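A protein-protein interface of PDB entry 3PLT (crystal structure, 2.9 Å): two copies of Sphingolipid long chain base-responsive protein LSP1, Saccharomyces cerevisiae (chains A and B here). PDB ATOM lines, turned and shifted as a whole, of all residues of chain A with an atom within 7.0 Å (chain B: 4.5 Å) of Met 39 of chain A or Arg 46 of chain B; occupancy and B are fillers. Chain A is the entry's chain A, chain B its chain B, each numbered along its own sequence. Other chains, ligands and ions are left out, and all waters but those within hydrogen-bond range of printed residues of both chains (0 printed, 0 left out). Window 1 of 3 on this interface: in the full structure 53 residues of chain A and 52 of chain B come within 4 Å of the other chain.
Met 39 of chain A touches just these residues of chain B: Val 42 (3.7 Å) and Arg 46 (3.5 Å). Arg 46 of chain B touches two residues of chain A. Printed residues of chain B within 4 Å of Leu 173 of chain A: Leu 78 (3.9 Å). Printed residues of chain B within 4 Å of Ala 38 of chain A: Val 42. Of the printed residues of chain A, Val 42 of chain B touches Ala 38 (3.3 Å) and Met 39 (3.7 Å). Of the printed residues of chain B, Thr 31 of chain A touches Glu 45 (3.6 Å), Glu 48 (3.99 Å) and Ala 49 (3.6 Å). Met 169 of chain A touches none of the printed residues of chain B. Arg 47 of chain B touches none of the printed residues of chain A. The nearest printed residue of chain B that does not touch Met 39 of chain A is Gln 82 of chain B (6.5 Å).
Among the printed residues, merely in contact across the chains: Leu 28 of chain A with Ala 49 of chain B (3.5 Å), Thr 31 of chain A with Glu 45 of chain B (3.6 Å), Thr 31 of chain A with Glu 48 of chain B (3.99 Å), Thr 31 of chain A with Ala 49 of chain B (3.6 Å), Glu 32 of chain A with Ala 49 of chain B (3.5 Å), Val 35 of chain A with Glu 45 of chain B (3.1 Å), Val 35 of chain A with Arg 46 of chain B (3.9 Å), Ala 38 of chain A with Val 42 of chain B (3.3 Å), Met 39 of chain A with Val 42 of chain B (3.7 Å) and Leu 173 of chain A with Leu 78 of chain B (3.9 Å).
The guanidinium group (NH2) of Arg 46 of chain B is in hydrogen-bond range of the side-chain sulfur (SD) of Met 39 of chain A (3.5 Å).
Of the 24 printed residues of chain A, 7 touch a printed residue of chain B. Printed residues of chain A that touch a printed residue of chain B: Leu 28, Thr 31, Glu 32, Val 35, Ala 38, Met 39 and Leu 173. Hydrophobic or aromatic side chains of chain A that line the printed part of chain B: Leu 28, Val 35, Ala 38, Met 39 and Leu 173. Printed residues of chain B that touch a printed residue of chain A: Val 42, Glu 45, Arg 46, Glu 48, Ala 49 and Leu 78. Hydrophobic or aromatic side chains of chain B within 4 Å of the printed part of chain A: Val 42, Ala 49 and Leu 78. Among the printed residues, 11 pairs touch across the chains. Among the printed residues, no Asp or Glu carboxylate lies within 4 Å of a Lys or Arg side-chain nitrogen of the other chain.
Positions printed for both chains: 42, 43, 44, 45 and 82. Of the 11 pairs that touch across the chains among the printed residues, none has its exchanged pair printed and touching as well.
OE1 of Gln 82 of chain B is in hydrogen-bond range of NH1 of Arg 46 of chain B (3.2 Å). The side-chain hydroxyl (OG) of Ser 44 of chain B sits at hydrogen-bond distance from the side-chain carboxylate (OE2) of Glu 45 of chain B (2.8 Å). The backbone carbonyl oxygen of Met 39 of chain A lies close to the side-chain amide oxygen of Gln 82 of chain A (3.2 Å). OE2 of Glu 32 of chain A sits close to OH of Tyr 89 of chain A, 3.4 Å away.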
ATOM      1  N   LEU A  28      27.966 -17.538  -4.419  1.00  0.00           N
ATOM      2  CA  LEU A  28      28.021 -18.591  -3.400  1.00  0.00           C
ATOM      3  C   LEU A  28      27.643 -18.058  -2.026  1.00  0.00           C
ATOM      4  O   LEU A  28      26.914 -18.694  -1.278  1.00  0.00           O
ATOM      5  CB  LEU A  28      29.431 -19.203  -3.349  1.00  0.00           C
ATOM      6  CG  LEU A  28      29.805 -19.994  -2.089  1.00  0.00           C
ATOM      7  CD1 LEU A  28      28.907 -21.212  -1.902  1.00  0.00           C
ATOM      8  CD2 LEU A  28      31.250 -20.388  -2.163  1.00  0.00           C
ATOM      9  N   THR A  31      23.875 -17.767  -2.070  1.00  0.00           N
ATOM     10  CA  THR A  31      23.223 -19.060  -1.947  1.00  0.00           C
ATOM     11  C   THR A  31      23.298 -19.536  -0.524  1.00  0.00           C
ATOM     12  O   THR A  31      22.330 -20.048  -0.004  1.00  0.00           O
ATOM     13  CB  THR A  31      23.820 -20.101  -2.903  1.00  0.00           C
ATOM     14  OG1 THR A  31      23.115 -20.041  -4.151  1.00  0.00           O
ATOM     15  CG2 THR A  31      23.699 -21.516  -2.338  1.00  0.00           C
ATOM     16  N   GLU A  32      24.444 -19.332   0.109  1.00  0.00           N
ATOM     17  CA  GLU A  32      24.647 -19.765   1.485  1.00  0.00           C
ATOM     18  C   GLU A  32      23.835 -18.962   2.507  1.00  0.00           C
ATOM     19  O   GLU A  32      23.468 -19.512   3.526  1.00  0.00           O
ATOM     20  CB  GLU A  32      26.135 -19.750   1.843  1.00  0.00           C
ATOM     21  CG  GLU A  32      26.956 -20.872   1.152  1.00  0.00           C
ATOM     22  CD  GLU A  32      26.948 -22.214   1.915  1.00  0.00           C
ATOM     23  OE1 GLU A  32      26.053 -22.402   2.785  1.00  0.00           O
ATOM     24  OE2 GLU A  32      27.843 -23.075   1.656  1.00  0.00           O
ATOM     25  N   GLY A  34      20.806 -18.117   1.912  1.00  0.00           N
ATOM     26  CA  GLY A  34      19.538 -18.817   1.755  1.00  0.00           C
ATOM     27  C   GLY A  34      19.472 -20.117   2.524  1.00  0.00           C
ATOM     28  O   GLY A  34      18.432 -20.439   3.098  1.00  0.00           O
ATOM     29  N   VAL A  35      20.581 -20.854   2.535  1.00  0.00           N
ATOM     30  CA  VAL A  35      20.679 -22.122   3.254  1.00  0.00           C
ATOM     31  C   VAL A  35      20.553 -21.895   4.739  1.00  0.00           C
ATOM     32  O   VAL A  35      19.863 -22.632   5.421  1.00  0.00           O
ATOM     33  CB  VAL A  35      22.026 -22.808   3.011  1.00  0.00           C
ATOM     34  CG1 VAL A  35      22.198 -24.056   3.915  1.00  0.00           C
ATOM     35  CG2 VAL A  35      22.191 -23.147   1.527  1.00  0.00           C
ATOM     36  N   LEU A  36      21.225 -20.872   5.244  1.00  0.00           N
ATOM     37  CA  LEU A  36      21.008 -20.440   6.619  1.00  0.00           C
ATOM     38  C   LEU A  36      19.502 -20.196   6.850  1.00  0.00           C
ATOM     39  O   LEU A  36      18.877 -20.884   7.662  1.00  0.00           O
ATOM     40  CB  LEU A  36      21.826 -19.174   6.929  1.00  0.00           C
ATOM     41  CG  LEU A  36      22.023 -18.817   8.406  1.00  0.00           C
ATOM     42  CD1 LEU A  36      22.998 -19.784   9.024  1.00  0.00           C
ATOM     43  CD2 LEU A  36      22.526 -17.382   8.586  1.00  0.00           C
ATOM     44  N   ARG A  37      18.922 -19.258   6.100  1.00  0.00           N
ATOM     45  CA  ARG A  37      17.519 -18.887   6.286  1.00  0.00           C
ATOM     46  C   ARG A  37      16.577 -20.092   6.360  1.00  0.00           C
ATOM     47  O   ARG A  37      15.615 -20.092   7.142  1.00  0.00           O
ATOM     48  CB  ARG A  37      17.048 -17.927   5.185  1.00  0.00           C
ATOM     49  CG  ARG A  37      17.333 -16.441   5.473  1.00  0.00           C
ATOM     50  CD  ARG A  37      16.429 -15.493   4.651  1.00  0.00           C
ATOM     51  NE  ARG A  37      16.194 -14.197   5.316  1.00  0.00           N
ATOM     52  CZ  ARG A  37      16.956 -13.105   5.191  1.00  0.00           C
ATOM     53  NH1 ARG A  37      18.046 -13.093   4.420  1.00  0.00           N
ATOM     54  NH2 ARG A  37      16.627 -12.004   5.855  1.00  0.00           N
ATOM     55  N   ALA A  38      16.853 -21.112   5.547  1.00  0.00           N
ATOM     56  CA  ALA A  38      16.029 -22.327   5.530  1.00  0.00           C
ATOM     57  C   ALA A  38      16.237 -23.181   6.780  1.00  0.00           C
ATOM     58  O   ALA A  38      15.274 -23.702   7.349  1.00  0.00           O
ATOM     59  CB  ALA A  38      16.308 -23.131   4.298  1.00  0.00           C
ATOM     60  N   MET A  39      17.494 -23.316   7.203  1.00  0.00           N
ATOM     61  CA  MET A  39      17.814 -24.065   8.414  1.00  0.00           C
ATOM     62  C   MET A  39      17.112 -23.471   9.641  1.00  0.00           C
ATOM     63  O   MET A  39      16.636 -24.220  10.493  1.00  0.00           O
ATOM     64  CB  MET A  39      19.329 -24.128   8.639  1.00  0.00           C
ATOM     65  CG  MET A  39      20.090 -24.942   7.590  1.00  0.00           C
ATOM     66  SD  MET A  39      21.708 -25.524   8.169  1.00  0.00           S
ATOM     67  CE  MET A  39      22.753 -24.105   7.862  1.00  0.00           C
ATOM     68  N   GLU A  40      17.048 -22.137   9.704  1.00  0.00           N
ATOM     69  CA  GLU A  40      16.296 -21.418  10.742  1.00  0.00           C
ATOM     70  C   GLU A  40      14.843 -21.870  10.857  1.00  0.00           C
ATOM     71  O   GLU A  40      14.338 -22.068  11.962  1.00  0.00           O
ATOM     72  CB  GLU A  40      16.284 -19.910  10.464  1.00  0.00           C
ATOM     73  CG  GLU A  40      17.612 -19.213  10.697  1.00  0.00           C
ATOM     74  CD  GLU A  40      17.517 -17.691  10.651  1.00  0.00           C
ATOM     75  OE1 GLU A  40      16.600 -17.115  11.275  1.00  0.00           O
ATOM     76  OE2 GLU A  40      18.384 -17.075  10.002  1.00  0.00           O
ATOM     77  N   VAL A  41      14.182 -21.995   9.707  1.00  0.00           N
ATOM     78  CA  VAL A  41      12.792 -22.418   9.638  1.00  0.00           C
ATOM     79  C   VAL A  41      12.638 -23.856  10.142  1.00  0.00           C
ATOM     80  O   VAL A  41      11.796 -24.143  10.998  1.00  0.00           O
ATOM     81  CB  VAL A  41      12.260 -22.299   8.196  1.00  0.00           C
ATOM     82  CG1 VAL A  41      10.890 -22.940   8.061  1.00  0.00           C
ATOM     83  CG2 VAL A  41      12.230 -20.843   7.767  1.00  0.00           C
ATOM     84  N   VAL A  42      13.463 -24.755   9.624  1.00  0.00           N
ATOM     85  CA  VAL A  42      13.452 -26.134  10.103  1.00  0.00           C
ATOM     86  C   VAL A  42      13.513 -26.143  11.630  1.00  0.00           C
ATOM     87  O   VAL A  42      12.585 -26.603  12.289  1.00  0.00           O
ATOM     88  CB  VAL A  42      14.629 -26.971   9.547  1.00  0.00           C
ATOM     89  CG1 VAL A  42      14.740 -28.270  10.299  1.00  0.00           C
ATOM     90  CG2 VAL A  42      14.458 -27.235   8.062  1.00  0.00           C
ATOM     91  N   ALA A  43      14.586 -25.600  12.192  1.00  0.00           N
ATOM     92  CA  ALA A  43      14.769 -25.620  13.642  1.00  0.00           C
ATOM     93  C   ALA A  43      13.545 -25.082  14.371  1.00  0.00           C
ATOM     94  O   ALA A  43      13.032 -25.723  15.282  1.00  0.00           O
ATOM     95  CB  ALA A  43      15.974 -24.829  14.021  1.00  0.00           C
ATOM     96  N   SER A  44      13.080 -23.904  13.953  1.00  0.00           N
ATOM     97  CA  SER A  44      11.853 -23.316  14.501  1.00  0.00           C
ATOM     98  C   SER A  44      10.683 -24.288  14.467  1.00  0.00           C
ATOM     99  O   SER A  44      10.061 -24.556  15.502  1.00  0.00           O
ATOM    100  CB  SER A  44      11.441 -22.061  13.734  1.00  0.00           C
ATOM    101  OG  SER A  44      10.051 -21.813  13.923  1.00  0.00           O
ATOM    102  N   GLU A  45      10.382 -24.802  13.277  1.00  0.00           N
ATOM    103  CA  GLU A  45       9.192 -25.617  13.106  1.00  0.00           C
ATOM    104  C   GLU A  45       9.333 -26.904  13.905  1.00  0.00           C
ATOM    105  O   GLU A  45       8.393 -27.314  14.596  1.00  0.00           O
ATOM    106  CB  GLU A  45       8.930 -25.917  11.635  1.00  0.00           C
ATOM    107  CG  GLU A  45       8.579 -24.698  10.806  1.00  0.00           C
ATOM    108  CD  GLU A  45       7.173 -24.160  11.060  1.00  0.00           C
ATOM    109  OE1 GLU A  45       6.190 -24.886  10.779  1.00  0.00           O
ATOM    110  OE2 GLU A  45       7.052 -22.995  11.511  1.00  0.00           O
ATOM    111  N   GLN A  82      20.167 -27.389  16.238  1.00  0.00           N
ATOM    112  CA  GLN A  82      20.237 -26.743  14.929  1.00  0.00           C
ATOM    113  C   GLN A  82      20.658 -25.305  15.118  1.00  0.00           C
ATOM    114  O   GLN A  82      21.626 -24.858  14.530  1.00  0.00           O
ATOM    115  CB  GLN A  82      18.892 -26.772  14.193  1.00  0.00           C
ATOM    116  CG  GLN A  82      18.685 -27.966  13.260  1.00  0.00           C
ATOM    117  CD  GLN A  82      18.898 -27.615  11.816  1.00  0.00           C
ATOM    118  OE1 GLN A  82      18.041 -26.980  11.180  1.00  0.00           O
ATOM    119  NE2 GLN A  82      20.049 -28.015  11.278  1.00  0.00           N
ATOM    120  N   ASP A  83      19.951 -24.574  15.962  1.00  0.00           N
ATOM    121  CA  ASP A  83      20.225 -23.150  16.063  1.00  0.00           C
ATOM    122  C   ASP A  83      21.637 -22.850  16.518  1.00  0.00           C
ATOM    123  O   ASP A  83      22.239 -21.881  16.064  1.00  0.00           O
ATOM    124  CB  ASP A  83      19.199 -22.448  16.936  1.00  0.00           C
ATOM    125  CG  ASP A  83      18.127 -21.750  16.111  1.00  0.00           C
ATOM    126  OD1 ASP A  83      17.635 -22.338  15.110  1.00  0.00           O
ATOM    127  OD2 ASP A  83      17.779 -20.598  16.461  1.00  0.00           O
ATOM    128  N   PHE A  85      24.121 -24.660  15.661  1.00  0.00           N
ATOM    129  CA  PHE A  85      24.893 -24.827  14.435  1.00  0.00           C
ATOM    130  C   PHE A  85      24.686 -23.684  13.447  1.00  0.00           C
ATOM    131  O   PHE A  85      25.591 -23.388  12.674  1.00  0.00           O
ATOM    132  CB  PHE A  85      24.591 -26.151  13.750  1.00  0.00           C
ATOM    133  CG  PHE A  85      25.207 -26.277  12.396  1.00  0.00           C
ATOM    134  CD1 PHE A  85      26.521 -26.674  12.253  1.00  0.00           C
ATOM    135  CD2 PHE A  85      24.473 -25.991  11.254  1.00  0.00           C
ATOM    136  CE1 PHE A  85      27.088 -26.793  10.990  1.00  0.00           C
ATOM    137  CE2 PHE A  85      25.036 -26.114   9.987  1.00  0.00           C
ATOM    138  CZ  PHE A  85      26.337 -26.510   9.857  1.00  0.00           C
ATOM    139  N   ILE A  86      23.515 -23.049  13.454  1.00  0.00           N
ATOM    140  CA  ILE A  86      23.322 -21.817  12.677  1.00  0.00           C
ATOM    141  C   ILE A  86      24.307 -20.702  13.079  1.00  0.00           C
ATOM    142  O   ILE A  86      25.092 -20.246  12.262  1.00  0.00           O
ATOM    143  CB  ILE A  86      21.879 -21.295  12.767  1.00  0.00           C
ATOM    144  CG1 ILE A  86      20.952 -22.147  11.897  1.00  0.00           C
ATOM    145  CG2 ILE A  86      21.812 -19.841  12.324  1.00  0.00           C
ATOM    146  CD1 ILE A  86      20.325 -23.301  12.600  1.00  0.00           C
ATOM    147  N   TYR A  89      27.457 -21.495  11.491  1.00  0.00           N
ATOM    148  CA  TYR A  89      27.369 -21.393  10.048  1.00  0.00           C
ATOM    149  C   TYR A  89      27.536 -19.929   9.682  1.00  0.00           C
ATOM    150  O   TYR A  89      28.307 -19.580   8.797  1.00  0.00           O
ATOM    151  CB  TYR A  89      26.023 -21.914   9.562  1.00  0.00           C
ATOM    152  CG  TYR A  89      26.016 -22.459   8.159  1.00  0.00           C
ATOM    153  CD1 TYR A  89      26.682 -23.638   7.854  1.00  0.00           C
ATOM    154  CD2 TYR A  89      25.302 -21.826   7.143  1.00  0.00           C
ATOM    155  CE1 TYR A  89      26.660 -24.170   6.562  1.00  0.00           C
ATOM    156  CE2 TYR A  89      25.273 -22.340   5.852  1.00  0.00           C
ATOM    157  CZ  TYR A  89      25.953 -23.516   5.570  1.00  0.00           C
ATOM    158  OH  TYR A  89      25.932 -24.043   4.295  1.00  0.00           O
ATOM    159  N   ASP A  90      26.840 -19.056  10.387  1.00  0.00           N
ATOM    160  CA  ASP A  90      26.967 -17.628  10.132  1.00  0.00           C
ATOM    161  C   ASP A  90      28.444 -17.200  10.068  1.00  0.00           C
ATOM    162  O   ASP A  90      28.859 -16.539   9.113  1.00  0.00           O
ATOM    163  CB  ASP A  90      26.213 -16.810  11.200  1.00  0.00           C
ATOM    164  CG  ASP A  90      25.749 -15.460  10.685  1.00  0.00           C
ATOM    165  OD1 ASP A  90      25.377 -15.378   9.492  1.00  0.00           O
ATOM    166  OD2 ASP A  90      25.742 -14.486  11.470  1.00  0.00           O
ATOM    167  N   MET A 169      33.487 -24.847  10.062  1.00  0.00           N
ATOM    168  CA  MET A 169      32.154 -25.349   9.703  1.00  0.00           C
ATOM    169  C   MET A 169      32.040 -26.874   9.792  1.00  0.00           C
ATOM    170  O   MET A 169      31.087 -27.376  10.372  1.00  0.00           O
ATOM    171  CB  MET A 169      31.768 -24.883   8.296  1.00  0.00           C
ATOM    172  CG  MET A 169      30.362 -25.272   7.859  1.00  0.00           C
ATOM    173  SD  MET A 169      30.266 -26.775   6.851  1.00  0.00           S
ATOM    174  CE  MET A 169      29.687 -26.126   5.289  1.00  0.00           C
ATOM    175  N   LEU A 173      29.560 -28.961  12.043  1.00  0.00           N
ATOM    176  CA  LEU A 173      28.607 -29.868  11.437  1.00  0.00           C
ATOM    177  C   LEU A 173      28.796 -31.262  11.990  1.00  0.00           C
ATOM    178  O   LEU A 173      27.819 -31.948  12.260  1.00  0.00           O
ATOM    179  CB  LEU A 173      28.770 -29.897   9.924  1.00  0.00           C
ATOM    180  CG  LEU A 173      27.761 -30.733   9.132  1.00  0.00           C
ATOM    181  CD1 LEU A 173      26.432 -30.029   9.102  1.00  0.00           C
ATOM    182  CD2 LEU A 173      28.289 -30.966   7.731  1.00  0.00           C
ATOM    183  N   LEU A 176      27.024 -31.120  15.470  1.00  0.00           N
ATOM    184  CA  LEU A 176      25.590 -31.250  15.236  1.00  0.00           C
ATOM    185  C   LEU A 176      25.249 -32.708  14.987  1.00  0.00           C
ATOM    186  O   LEU A 176      24.556 -33.335  15.777  1.00  0.00           O
ATOM    187  CB  LEU A 176      25.149 -30.424  14.022  1.00  0.00           C
ATOM    188  CG  LEU A 176      23.649 -30.336  13.725  1.00  0.00           C
ATOM    189  CD1 LEU A 176      22.947 -29.602  14.858  1.00  0.00           C
ATOM    190  CD2 LEU A 176      23.412 -29.625  12.391  1.00  0.00           C
ATOM    191  N   VAL B  42      16.750 -26.664   2.036  1.00  0.00           N
ATOM    192  CA  VAL B  42      18.107 -26.783   2.511  1.00  0.00           C
ATOM    193  C   VAL B  42      18.934 -27.726   1.643  1.00  0.00           C
ATOM    194  O   VAL B  42      20.028 -27.372   1.235  1.00  0.00           O
ATOM    195  CB  VAL B  42      18.151 -27.216   3.967  1.00  0.00           C
ATOM    196  CG1 VAL B  42      19.588 -27.489   4.401  1.00  0.00           C
ATOM    197  CG2 VAL B  42      17.510 -26.135   4.848  1.00  0.00           C
ATOM    198  N   ALA B  43      18.422 -28.908   1.335  1.00  0.00           N
ATOM    199  CA  ALA B  43      19.145 -29.800   0.424  1.00  0.00           C
ATOM    200  C   ALA B  43      19.412 -29.101  -0.907  1.00  0.00           C
ATOM    201  O   ALA B  43      20.542 -28.983  -1.344  1.00  0.00           O
ATOM    202  CB  ALA B  43      18.382 -31.080   0.192  1.00  0.00           C
ATOM    203  N   SER B  44      18.355 -28.624  -1.538  1.00  0.00           N
ATOM    204  CA  SER B  44      18.458 -27.918  -2.801  1.00  0.00           C
ATOM    205  C   SER B  44      19.615 -26.942  -2.843  1.00  0.00           C
ATOM    206  O   SER B  44      20.453 -27.003  -3.741  1.00  0.00           O
ATOM    207  CB  SER B  44      17.176 -27.142  -3.060  1.00  0.00           C
ATOM    208  OG  SER B  44      17.467 -25.901  -3.687  1.00  0.00           O
ATOM    209  N   GLU B  45      19.638 -26.029  -1.879  1.00  0.00           N
ATOM    210  CA  GLU B  45      20.625 -24.960  -1.858  1.00  0.00           C
ATOM    211  C   GLU B  45      22.018 -25.500  -1.577  1.00  0.00           C
ATOM    212  O   GLU B  45      22.994 -25.095  -2.216  1.00  0.00           O
ATOM    213  CB  GLU B  45      20.272 -23.908  -0.807  1.00  0.00           C
ATOM    214  CG  GLU B  45      18.941 -23.203  -0.991  1.00  0.00           C
ATOM    215  CD  GLU B  45      18.795 -22.552  -2.345  1.00  0.00           C
ATOM    216  OE1 GLU B  45      19.060 -21.330  -2.456  1.00  0.00           O
ATOM    217  OE2 GLU B  45      18.415 -23.271  -3.295  1.00  0.00           O
ATOM    218  N   ARG B  46      22.129 -26.412  -0.625  1.00  0.00           N
ATOM    219  CA  ARG B  46      23.433 -27.000  -0.360  1.00  0.00           C
ATOM    220  C   ARG B  46      24.049 -27.405  -1.689  1.00  0.00           C
ATOM    221  O   ARG B  46      25.207 -27.122  -1.957  1.00  0.00           O
ATOM    222  CB  ARG B  46      23.340 -28.204   0.577  1.00  0.00           C
ATOM    223  CG  ARG B  46      24.161 -28.030   1.850  1.00  0.00           C
ATOM    224  CD  ARG B  46      23.688 -28.945   2.957  1.00  0.00           C
ATOM    225  NE  ARG B  46      23.822 -28.332   4.275  1.00  0.00           N
ATOM    226  CZ  ARG B  46      23.249 -28.796   5.389  1.00  0.00           C
ATOM    227  NH1 ARG B  46      22.484 -29.896   5.368  1.00  0.00           N
ATOM    228  NH2 ARG B  46      23.433 -28.153   6.543  1.00  0.00           N
ATOM    229  N   ARG B  47      23.245 -28.023  -2.540  1.00  0.00           N
ATOM    230  CA  ARG B  47      23.718 -28.456  -3.845  1.00  0.00           C
ATOM    231  C   ARG B  47      24.164 -27.313  -4.722  1.00  0.00           C
ATOM    232  O   ARG B  47      25.132 -27.441  -5.462  1.00  0.00           O
ATOM    233  CB  ARG B  47      22.646 -29.264  -4.568  1.00  0.00           C
ATOM    234  CG  ARG B  47      22.322 -30.558  -3.851  1.00  0.00           C
ATOM    235  CD  ARG B  47      21.647 -31.563  -4.764  1.00  0.00           C
ATOM    236  NE  ARG B  47      20.609 -32.278  -4.029  1.00  0.00           N
ATOM    237  CZ  ARG B  47      19.319 -31.958  -4.042  1.00  0.00           C
ATOM    238  NH1 ARG B  47      18.862 -30.948  -4.776  1.00  0.00           N
ATOM    239  NH2 ARG B  47      18.472 -32.665  -3.324  1.00  0.00           N
ATOM    240  N   GLU B  48      23.463 -26.199  -4.660  1.00  0.00           N
ATOM    241  CA  GLU B  48      23.903 -25.045  -5.399  1.00  0.00           C
ATOM    242  C   GLU B  48      25.213 -24.562  -4.791  1.00  0.00           C
ATOM    243  O   GLU B  48      26.163 -24.281  -5.505  1.00  0.00           O
ATOM    244  CB  GLU B  48      22.837 -23.955  -5.378  1.00  0.00           C
ATOM    245  CG  GLU B  48      22.531 -23.403  -6.750  1.00  0.00           C
ATOM    246  CD  GLU B  48      21.980 -24.465  -7.692  1.00  0.00           C
ATOM    247  OE1 GLU B  48      21.463 -25.490  -7.173  1.00  0.00           O
ATOM    248  OE2 GLU B  48      22.067 -24.271  -8.938  1.00  0.00           O
ATOM    249  N   ALA B  49      25.269 -24.498  -3.468  1.00  0.00           N
ATOM    250  CA  ALA B  49      26.486 -24.089  -2.785  1.00  0.00           C
ATOM    251  C   ALA B  49      27.696 -24.915  -3.214  1.00  0.00           C
ATOM    252  O   ALA B  49      28.766 -24.378  -3.463  1.00  0.00           O
ATOM    253  CB  ALA B  49      26.302 -24.175  -1.293  1.00  0.00           C
ATOM    254  N   ALA B  50      27.529 -26.224  -3.304  1.00  0.00           N
ATOM    255  CA  ALA B  50      28.630 -27.098  -3.718  1.00  0.00           C
ATOM    256  C   ALA B  50      29.135 -26.671  -5.077  1.00  0.00           C
ATOM    257  O   ALA B  50      30.306 -26.347  -5.242  1.00  0.00           O
ATOM    258  CB  ALA B  50      28.187 -28.539  -3.764  1.00  0.00           C
ATOM    259  N   ILE B  75      30.095 -32.073  -0.349  1.00  0.00           N
ATOM    260  CA  ILE B  75      28.945 -31.246   0.011  1.00  0.00           C
ATOM    261  C   ILE B  75      27.720 -31.563  -0.841  1.00  0.00           C
ATOM    262  O   ILE B  75      26.612 -31.608  -0.325  1.00  0.00           O
ATOM    263  CB  ILE B  75      29.300 -29.739  -0.053  1.00  0.00           C
ATOM    264  CG1 ILE B  75      30.252 -29.393   1.095  1.00  0.00           C
ATOM    265  CG2 ILE B  75      28.063 -28.877   0.022  1.00  0.00           C
ATOM    266  CD1 ILE B  75      31.072 -28.194   0.845  1.00  0.00           C
ATOM    267  N   LEU B  78      25.975 -34.360   0.740  1.00  0.00           N
ATOM    268  CA  LEU B  78      25.204 -33.949   1.915  1.00  0.00           C
ATOM    269  C   LEU B  78      23.787 -33.721   1.434  1.00  0.00           C
ATOM    270  O   LEU B  78      22.841 -34.322   1.936  1.00  0.00           O
ATOM    271  CB  LEU B  78      25.755 -32.667   2.554  1.00  0.00           C
ATOM    272  CG  LEU B  78      27.004 -32.775   3.441  1.00  0.00           C
ATOM    273  CD1 LEU B  78      27.500 -31.427   3.949  1.00  0.00           C
ATOM    274  CD2 LEU B  78      26.669 -33.658   4.599  1.00  0.00           C
ATOM    275  N   GLN B  82      20.358 -35.813   2.226  1.00  0.00           N
ATOM    276  CA  GLN B  82      19.226 -35.090   2.783  1.00  0.00           C
ATOM    277  C   GLN B  82      17.947 -35.414   2.041  1.00  0.00           C
ATOM    278  O   GLN B  82      16.949 -35.756   2.668  1.00  0.00           O
ATOM    279  CB  GLN B  82      19.466 -33.586   2.792  1.00  0.00           C
ATOM    280  CG  GLN B  82      18.760 -32.910   3.949  1.00  0.00           C
ATOM    281  CD  GLN B  82      19.229 -31.497   4.189  1.00  0.00           C
ATOM    282  OE1 GLN B  82      20.145 -31.016   3.526  1.00  0.00           O
ATOM    283  NE2 GLN B  82      18.600 -30.821   5.145  1.00  0.00           N
ATOM    284  N   PHE B 180      26.438 -37.970   7.681  1.00  0.00           N
ATOM    285  CA  PHE B 180      26.908 -36.585   7.700  1.00  0.00           C
ATOM    286  C   PHE B 180      28.212 -36.513   8.442  1.00  0.00           C
ATOM    287  O   PHE B 180      29.194 -35.963   7.936  1.00  0.00           O
ATOM    288  CB  PHE B 180      25.917 -35.648   8.385  1.00  0.00           C
ATOM    289  CG  PHE B 180      25.015 -34.920   7.438  1.00  0.00           C
ATOM    290  CD1 PHE B 180      24.792 -33.563   7.586  1.00  0.00           C
ATOM    291  CD2 PHE B 180      24.386 -35.584   6.402  1.00  0.00           C
ATOM    292  CE1 PHE B 180      23.962 -32.886   6.727  1.00  0.00           C
ATOM    293  CE2 PHE B 180      23.555 -34.900   5.543  1.00  0.00           C
ATOM    294  CZ  PHE B 180      23.343 -33.549   5.711  1.00  0.00           C
